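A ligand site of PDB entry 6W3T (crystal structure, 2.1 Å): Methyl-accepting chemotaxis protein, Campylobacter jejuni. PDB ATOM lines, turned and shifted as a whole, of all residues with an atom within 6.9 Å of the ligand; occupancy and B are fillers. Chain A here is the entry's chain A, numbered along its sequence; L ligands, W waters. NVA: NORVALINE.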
ATOM      1  N   ASN A  80      18.218  15.888  -0.727  1.00  0.00           N
ATOM      2  CA  ASN A  80      16.921  15.262  -0.986  1.00  0.00           C
ATOM      3  C   ASN A  80      16.753  15.045  -2.480  1.00  0.00           C
ATOM      4  O   ASN A  80      17.164  15.905  -3.273  1.00  0.00           O
ATOM      5  CB  ASN A  80      15.737  16.105  -0.533  1.00  0.00           C
ATOM      6  CG  ASN A  80      15.794  16.478   0.912  1.00  0.00           C
ATOM      7  OD1 ASN A  80      15.718  15.606   1.785  1.00  0.00           O
ATOM      8  ND2 ASN A  80      15.900  17.781   1.191  1.00  0.00           N
ATOM      9  N   TYR A  82      13.348  13.631  -4.946  1.00  0.00           N
ATOM     10  CA  TYR A  82      11.951  13.307  -4.714  1.00  0.00           C
ATOM     11  C   TYR A  82      11.134  13.452  -5.998  1.00  0.00           C
ATOM     12  O   TYR A  82      11.564  14.099  -6.965  1.00  0.00           O
ATOM     13  CB  TYR A  82      11.350  14.168  -3.600  1.00  0.00           C
ATOM     14  CG  TYR A  82      11.759  15.634  -3.633  1.00  0.00           C
ATOM     15  CD1 TYR A  82      12.972  16.056  -3.081  1.00  0.00           C
ATOM     16  CD2 TYR A  82      10.937  16.574  -4.229  1.00  0.00           C
ATOM     17  CE1 TYR A  82      13.348  17.397  -3.114  1.00  0.00           C
ATOM     18  CE2 TYR A  82      11.293  17.916  -4.271  1.00  0.00           C
ATOM     19  CZ  TYR A  82      12.503  18.314  -3.715  1.00  0.00           C
ATOM     20  OH  TYR A  82      12.843  19.645  -3.767  1.00  0.00           O
ATOM     21  N   VAL A  90       4.392  13.124  -2.073  1.00  0.00           N
ATOM     22  CA  VAL A  90       5.731  13.146  -2.648  1.00  0.00           C
ATOM     23  C   VAL A  90       6.486  11.919  -2.180  1.00  0.00           C
ATOM     24  O   VAL A  90       6.517  11.610  -0.977  1.00  0.00           O
ATOM     25  CB  VAL A  90       6.484  14.456  -2.280  1.00  0.00           C
ATOM     26  CG1 VAL A  90       6.508  14.680  -0.767  1.00  0.00           C
ATOM     27  CG2 VAL A  90       7.912  14.474  -2.871  1.00  0.00           C
ATOM     28  N   LEU A  91       7.060  11.171  -3.129  1.00  0.00           N
ATOM     29  CA  LEU A  91       7.993  10.094  -2.804  1.00  0.00           C
ATOM     30  C   LEU A  91       9.360  10.727  -2.525  1.00  0.00           C
ATOM     31  O   LEU A  91       9.949  11.346  -3.413  1.00  0.00           O
ATOM     32  CB  LEU A  91       8.090   9.104  -3.960  1.00  0.00           C
ATOM     33  CG  LEU A  91       9.064   7.961  -3.779  1.00  0.00           C
ATOM     34  CD1 LEU A  91       8.623   7.059  -2.622  1.00  0.00           C
ATOM     35  CD2 LEU A  91       9.220   7.163  -5.087  1.00  0.00           C
ATOM     36  N   LEU A  92       9.880  10.567  -1.300  1.00  0.00           N
ATOM     37  CA  LEU A  92      11.012  11.347  -0.814  1.00  0.00           C
ATOM     38  C   LEU A  92      12.175  10.433  -0.470  1.00  0.00           C
ATOM     39  O   LEU A  92      12.035   9.543   0.367  1.00  0.00           O
ATOM     40  CB  LEU A  92      10.603  12.164   0.415  1.00  0.00           C
ATOM     41  CG  LEU A  92      11.718  12.896   1.173  1.00  0.00           C
ATOM     42  CD1 LEU A  92      12.422  13.925   0.290  1.00  0.00           C
ATOM     43  CD2 LEU A  92      11.175  13.531   2.443  1.00  0.00           C
ATOM     44  N   LEU A 108       3.576  17.579   3.104  1.00  0.00           N
ATOM     45  CA  LEU A 108       4.572  18.592   2.749  1.00  0.00           C
ATOM     46  C   LEU A 108       4.039  19.677   1.823  1.00  0.00           C
ATOM     47  O   LEU A 108       4.838  20.481   1.314  1.00  0.00           O
ATOM     48  CB  LEU A 108       5.804  17.915   2.131  1.00  0.00           C
ATOM     49  CG  LEU A 108       6.535  16.959   3.076  1.00  0.00           C
ATOM     50  CD1 LEU A 108       7.706  16.259   2.414  1.00  0.00           C
ATOM     51  CD2 LEU A 108       7.002  17.702   4.306  1.00  0.00           C
ATOM     52  N   ASP A 109       2.722  19.730   1.573  1.00  0.00           N
ATOM     53  CA  ASP A 109       2.087  20.849   0.867  1.00  0.00           C
ATOM     54  C   ASP A 109       2.766  21.178  -0.461  1.00  0.00           C
ATOM     55  O   ASP A 109       2.899  22.353  -0.824  1.00  0.00           O
ATOM     56  CB  ASP A 109       2.030  22.100   1.750  1.00  0.00           C
ATOM     57  CG  ASP A 109       1.053  21.970   2.880  1.00  0.00           C
ATOM     58  OD1 ASP A 109      -0.167  21.932   2.616  1.00  0.00           O
ATOM     59  OD2 ASP A 109       1.512  21.917   4.045  1.00  0.00           O
ATOM     60  N   ILE A 110       3.167  20.146  -1.207  1.00  0.00           N
ATOM     61  CA  ILE A 110       4.083  20.359  -2.329  1.00  0.00           C
ATOM     62  C   ILE A 110       3.475  21.274  -3.379  1.00  0.00           C
ATOM     63  O   ILE A 110       4.192  21.982  -4.080  1.00  0.00           O
ATOM     64  CB  ILE A 110       4.531  19.016  -2.940  1.00  0.00           C
ATOM     65  CG1 ILE A 110       3.381  18.365  -3.716  1.00  0.00           C
ATOM     66  CG2 ILE A 110       5.072  18.104  -1.865  1.00  0.00           C
ATOM     67  CD1 ILE A 110       3.669  16.958  -4.148  1.00  0.00           C
ATOM     68  N   LYS A 113       4.622  24.814  -3.323  1.00  0.00           N
ATOM     69  CA  LYS A 113       6.041  25.075  -3.476  1.00  0.00           C
ATOM     70  C   LYS A 113       6.347  25.561  -4.886  1.00  0.00           C
ATOM     71  O   LYS A 113       5.836  25.013  -5.874  1.00  0.00           O
ATOM     72  CB  LYS A 113       6.839  23.806  -3.155  1.00  0.00           C
ATOM     73  CG  LYS A 113       6.573  23.296  -1.739  1.00  0.00           C
ATOM     74  CD  LYS A 113       7.164  24.244  -0.699  1.00  0.00           C
ATOM     75  CE  LYS A 113       6.642  23.954   0.712  1.00  0.00           C
ATOM     76  NZ  LYS A 113       7.171  22.702   1.268  1.00  0.00           N
ATOM     77  N   TRP A 115       9.100  25.185  -6.505  1.00  0.00           N
ATOM     78  CA  TRP A 115       9.762  24.153  -7.297  1.00  0.00           C
ATOM     79  C   TRP A 115       8.740  23.237  -7.955  1.00  0.00           C
ATOM     80  O   TRP A 115       8.982  22.739  -9.061  1.00  0.00           O
ATOM     81  CB  TRP A 115      10.741  23.342  -6.441  1.00  0.00           C
ATOM     82  CG  TRP A 115      10.112  22.516  -5.343  1.00  0.00           C
ATOM     83  CD1 TRP A 115      10.101  22.809  -3.994  1.00  0.00           C
ATOM     84  CD2 TRP A 115       9.417  21.264  -5.476  1.00  0.00           C
ATOM     85  NE1 TRP A 115       9.436  21.825  -3.295  1.00  0.00           N
ATOM     86  CE2 TRP A 115       9.009  20.870  -4.182  1.00  0.00           C
ATOM     87  CE3 TRP A 115       9.099  20.436  -6.565  1.00  0.00           C
ATOM     88  CZ2 TRP A 115       8.298  19.687  -3.947  1.00  0.00           C
ATOM     89  CZ3 TRP A 115       8.382  19.273  -6.335  1.00  0.00           C
ATOM     90  CH2 TRP A 115       7.987  18.907  -5.042  1.00  0.00           C
ATOM     91  N   TYR A 131      17.013  28.481  -0.507  1.00  0.00           N
ATOM     92  CA  TYR A 131      15.907  28.610   0.431  1.00  0.00           C
ATOM     93  C   TYR A 131      16.022  27.499   1.453  1.00  0.00           C
ATOM     94  O   TYR A 131      16.758  26.532   1.257  1.00  0.00           O
ATOM     95  CB  TYR A 131      14.540  28.567  -0.267  1.00  0.00           C
ATOM     96  CG  TYR A 131      14.203  27.181  -0.776  1.00  0.00           C
ATOM     97  CD1 TYR A 131      14.696  26.733  -1.992  1.00  0.00           C
ATOM     98  CD2 TYR A 131      13.415  26.321  -0.031  1.00  0.00           C
ATOM     99  CE1 TYR A 131      14.412  25.459  -2.458  1.00  0.00           C
ATOM    100  CE2 TYR A 131      13.125  25.057  -0.481  1.00  0.00           C
ATOM    101  CZ  TYR A 131      13.623  24.626  -1.695  1.00  0.00           C
ATOM    102  OH  TYR A 131      13.330  23.368  -2.138  1.00  0.00           O
ATOM    103  N   LEU A 132      15.313  27.650   2.559  1.00  0.00           N
ATOM    104  CA  LEU A 132      15.419  26.692   3.660  1.00  0.00           C
ATOM    105  C   LEU A 132      14.555  25.472   3.341  1.00  0.00           C
ATOM    106  O   LEU A 132      13.329  25.563   3.289  1.00  0.00           O
ATOM    107  CB  LEU A 132      14.980  27.353   4.964  1.00  0.00           C
ATOM    108  CG  LEU A 132      15.189  26.531   6.237  1.00  0.00           C
ATOM    109  CD1 LEU A 132      16.660  26.288   6.447  1.00  0.00           C
ATOM    110  CD2 LEU A 132      14.589  27.269   7.426  1.00  0.00           C
ATOM    111  N   ASP A 133      15.204  24.319   3.167  1.00  0.00           N
ATOM    112  CA  ASP A 133      14.489  23.065   2.939  1.00  0.00           C
ATOM    113  C   ASP A 133      13.584  22.705   4.118  1.00  0.00           C
ATOM    114  O   ASP A 133      14.015  22.742   5.273  1.00  0.00           O
ATOM    115  CB  ASP A 133      15.507  21.947   2.697  1.00  0.00           C
ATOM    116  CG  ASP A 133      14.885  20.580   2.723  1.00  0.00           C
ATOM    117  OD1 ASP A 133      13.799  20.419   2.134  1.00  0.00           O
ATOM    118  OD2 ASP A 133      15.505  19.665   3.330  1.00  0.00           O
ATOM    119  N   THR A 134      12.340  22.316   3.812  1.00  0.00           N
ATOM    120  CA  THR A 134      11.418  21.889   4.879  1.00  0.00           C
ATOM    121  C   THR A 134      11.844  20.568   5.511  1.00  0.00           C
ATOM    122  O   THR A 134      11.620  20.359   6.703  1.00  0.00           O
ATOM    123  CB  THR A 134       9.982  21.739   4.346  1.00  0.00           C
ATOM    124  OG1 THR A 134       9.665  22.827   3.471  1.00  0.00           O
ATOM    125  CG2 THR A 134       9.001  21.733   5.502  1.00  0.00           C
ATOM    126  N   VAL A 135      12.438  19.671   4.727  1.00  0.00           N
ATOM    127  CA  VAL A 135      12.663  18.305   5.215  1.00  0.00           C
ATOM    128  C   VAL A 135      13.832  18.264   6.195  1.00  0.00           C
ATOM    129  O   VAL A 135      13.701  17.721   7.300  1.00  0.00           O
ATOM    130  CB  VAL A 135      12.871  17.343   4.029  1.00  0.00           C
ATOM    131  CG1 VAL A 135      13.202  15.936   4.547  1.00  0.00           C
ATOM    132  CG2 VAL A 135      11.622  17.338   3.129  1.00  0.00           C
ATOM    133  N   LEU A 136      14.983  18.797   5.828  1.00  0.00           N
ATOM    134  CA  LEU A 136      16.156  18.698   6.685  1.00  0.00           C
ATOM    135  C   LEU A 136      16.657  20.034   7.211  1.00  0.00           C
ATOM    136  O   LEU A 136      17.689  20.065   7.899  1.00  0.00           O
ATOM    137  CB  LEU A 136      17.293  17.964   5.957  1.00  0.00           C
ATOM    138  CG  LEU A 136      16.936  16.509   5.631  1.00  0.00           C
ATOM    139  CD1 LEU A 136      18.000  15.901   4.724  1.00  0.00           C
ATOM    140  CD2 LEU A 136      16.783  15.688   6.900  1.00  0.00           C
ATOM    141  N   GLN A 138      18.076  22.691   5.947  1.00  0.00           N
ATOM    142  CA  GLN A 138      19.325  23.241   5.424  1.00  0.00           C
ATOM    143  C   GLN A 138      19.001  24.077   4.188  1.00  0.00           C
ATOM    144  O   GLN A 138      17.994  23.841   3.514  1.00  0.00           O
ATOM    145  CB  GLN A 138      20.315  22.148   5.076  1.00  0.00           C
ATOM    146  CG  GLN A 138      20.596  21.216   6.237  1.00  0.00           C
ATOM    147  CD  GLN A 138      21.592  20.132   5.898  1.00  0.00           C
ATOM    148  OE1 GLN A 138      22.452  20.322   5.042  1.00  0.00           O
ATOM    149  NE2 GLN A 138      21.490  19.004   6.572  1.00  0.00           N
ATOM    150  N   VAL A 140      19.174  25.127   0.475  1.00  0.00           N
ATOM    151  CA  VAL A 140      19.367  24.304  -0.713  1.00  0.00           C
ATOM    152  C   VAL A 140      19.045  25.105  -1.962  1.00  0.00           C
ATOM    153  O   VAL A 140      18.295  26.082  -1.944  1.00  0.00           O
ATOM    154  CB  VAL A 140      18.506  23.020  -0.705  1.00  0.00           C
ATOM    155  CG1 VAL A 140      18.691  22.235   0.572  1.00  0.00           C
ATOM    156  CG2 VAL A 140      17.051  23.366  -0.906  1.00  0.00           C
ATOM    157  N   THR A 142      17.246  24.001  -5.456  1.00  0.00           N
ATOM    158  CA  THR A 142      16.437  22.910  -5.975  1.00  0.00           C
ATOM    159  C   THR A 142      16.382  22.963  -7.491  1.00  0.00           C
ATOM    160  O   THR A 142      16.138  24.018  -8.085  1.00  0.00           O
ATOM    161  CB  THR A 142      15.006  22.939  -5.405  1.00  0.00           C
ATOM    162  OG1 THR A 142      15.055  22.634  -4.007  1.00  0.00           O
ATOM    163  CG2 THR A 142      14.127  21.878  -6.124  1.00  0.00           C
ATOM    164  N   ASP A 160      17.553  18.510  -4.403  1.00  0.00           N
ATOM    165  CA  ASP A 160      18.028  19.571  -3.511  1.00  0.00           C
ATOM    166  C   ASP A 160      19.535  19.420  -3.327  1.00  0.00           C
ATOM    167  O   ASP A 160      20.002  18.394  -2.813  1.00  0.00           O
ATOM    168  CB  ASP A 160      17.337  19.514  -2.149  1.00  0.00           C
ATOM    169  CG  ASP A 160      15.837  19.758  -2.218  1.00  0.00           C
ATOM    170  OD1 ASP A 160      15.330  20.248  -3.262  1.00  0.00           O
ATOM    171  OD2 ASP A 160      15.177  19.482  -1.189  1.00  0.00           O
HETATM  172  N   NVA L   1      13.261  21.050  -0.339  1.00  0.00           N
HETATM  173  CA  NVA L   1      11.872  20.770  -0.724  1.00  0.00           C
HETATM  174  CB  NVA L   1      11.415  19.356  -0.349  1.00  0.00           C
HETATM  175  CG  NVA L   1      10.118  18.830  -0.973  1.00  0.00           C
HETATM  176  CD  NVA L   1      10.014  17.376  -0.593  1.00  0.00           C
HETATM  177  C   NVA L   1      10.989  21.750   0.023  1.00  0.00           C
HETATM  178  O   NVA L   1      11.289  22.411   1.020  1.00  0.00           O
HETATM  179  OXT NVA L   1       9.732  21.884  -0.505  1.00  0.00           O
HETATM  180  O   HOH W   1       9.835  25.045   1.908  1.00  0.00           O
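The side-chain carboxylate of Asp 133 is in salt-bridge range of a nitrogen (N) of the ligand, at 2.6 Å. OD2 of Asp 160 is in salt-bridge range of N of the ligand (2.6 Å). The side-chain hydroxyl of Tyr 131 sits at hydrogen-bond distance from a nitrogen (N) of the ligand (2.9 Å). An oxygen (O) of the ligand sits at hydrogen-bond distance from the backbone NH of Thr 134, at 3.0 Å. The side-chain amino group (NZ) of Lys 113 lies within salt-bridge range of an oxygen (OXT) of the ligand (3.2 Å). The side-chain hydroxyl of Thr 134 is in hydrogen-bond range of an oxygen (O) of the ligand, at 3.0 Å. The indole nitrogen (NE1) of Trp 115 lies within hydrogen-bond range of an oxygen (OXT) of the ligand (2.8 Å).
The backbone NH (N) of Leu 136 lies within hydrogen-bond range of the side-chain carboxylate (OD2) of Asp 133. The side-chain hydroxyl (OH) of Tyr 82 is in hydrogen-bond range of the side-chain carboxylate (OD1) of Asp 160 (2.6 Å). The backbone NH (N) of Asp 133 sits at hydrogen-bond distance from the backbone carbonyl oxygen (O) of Gln 138 (2.9 Å). N of Val 135 sits at hydrogen-bond distance from OD1 of Asp 133, 3.0 Å away. The backbone carbonyl oxygen of Leu 108 sits at hydrogen-bond distance from the side-chain amino group of Lys 113 (3.2 Å). O of Tyr 131 lies within hydrogen-bond range of N of Val 140 (2.9 Å). The side-chain hydroxyl of Thr 134 is in hydrogen-bond range of the side-chain amino group of Lys 113, 3.3 Å away. The side-chain amide nitrogen (ND2) of Asn 80 is in hydrogen-bond range of the side-chain carboxylate (OD2) of Asp 133, 2.9 Å away.
OH of Tyr 82 touches CA of the ligand, at 3.4 Å. Leu 108 touches the ligand. Hydrophobic or aromatic side chains that line the ligand: Tyr 82, Leu 108, Trp 115 and Tyr 131. The nearest printed residue that does not touch the ligand is Val 135 (4.03 Å).
Water W1 lies within hydrogen-bond range of the side-chain hydroxyl (OG1) of Thr 134 (2.7 Å) and an oxygen (O) of the ligand (3.1 Å).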
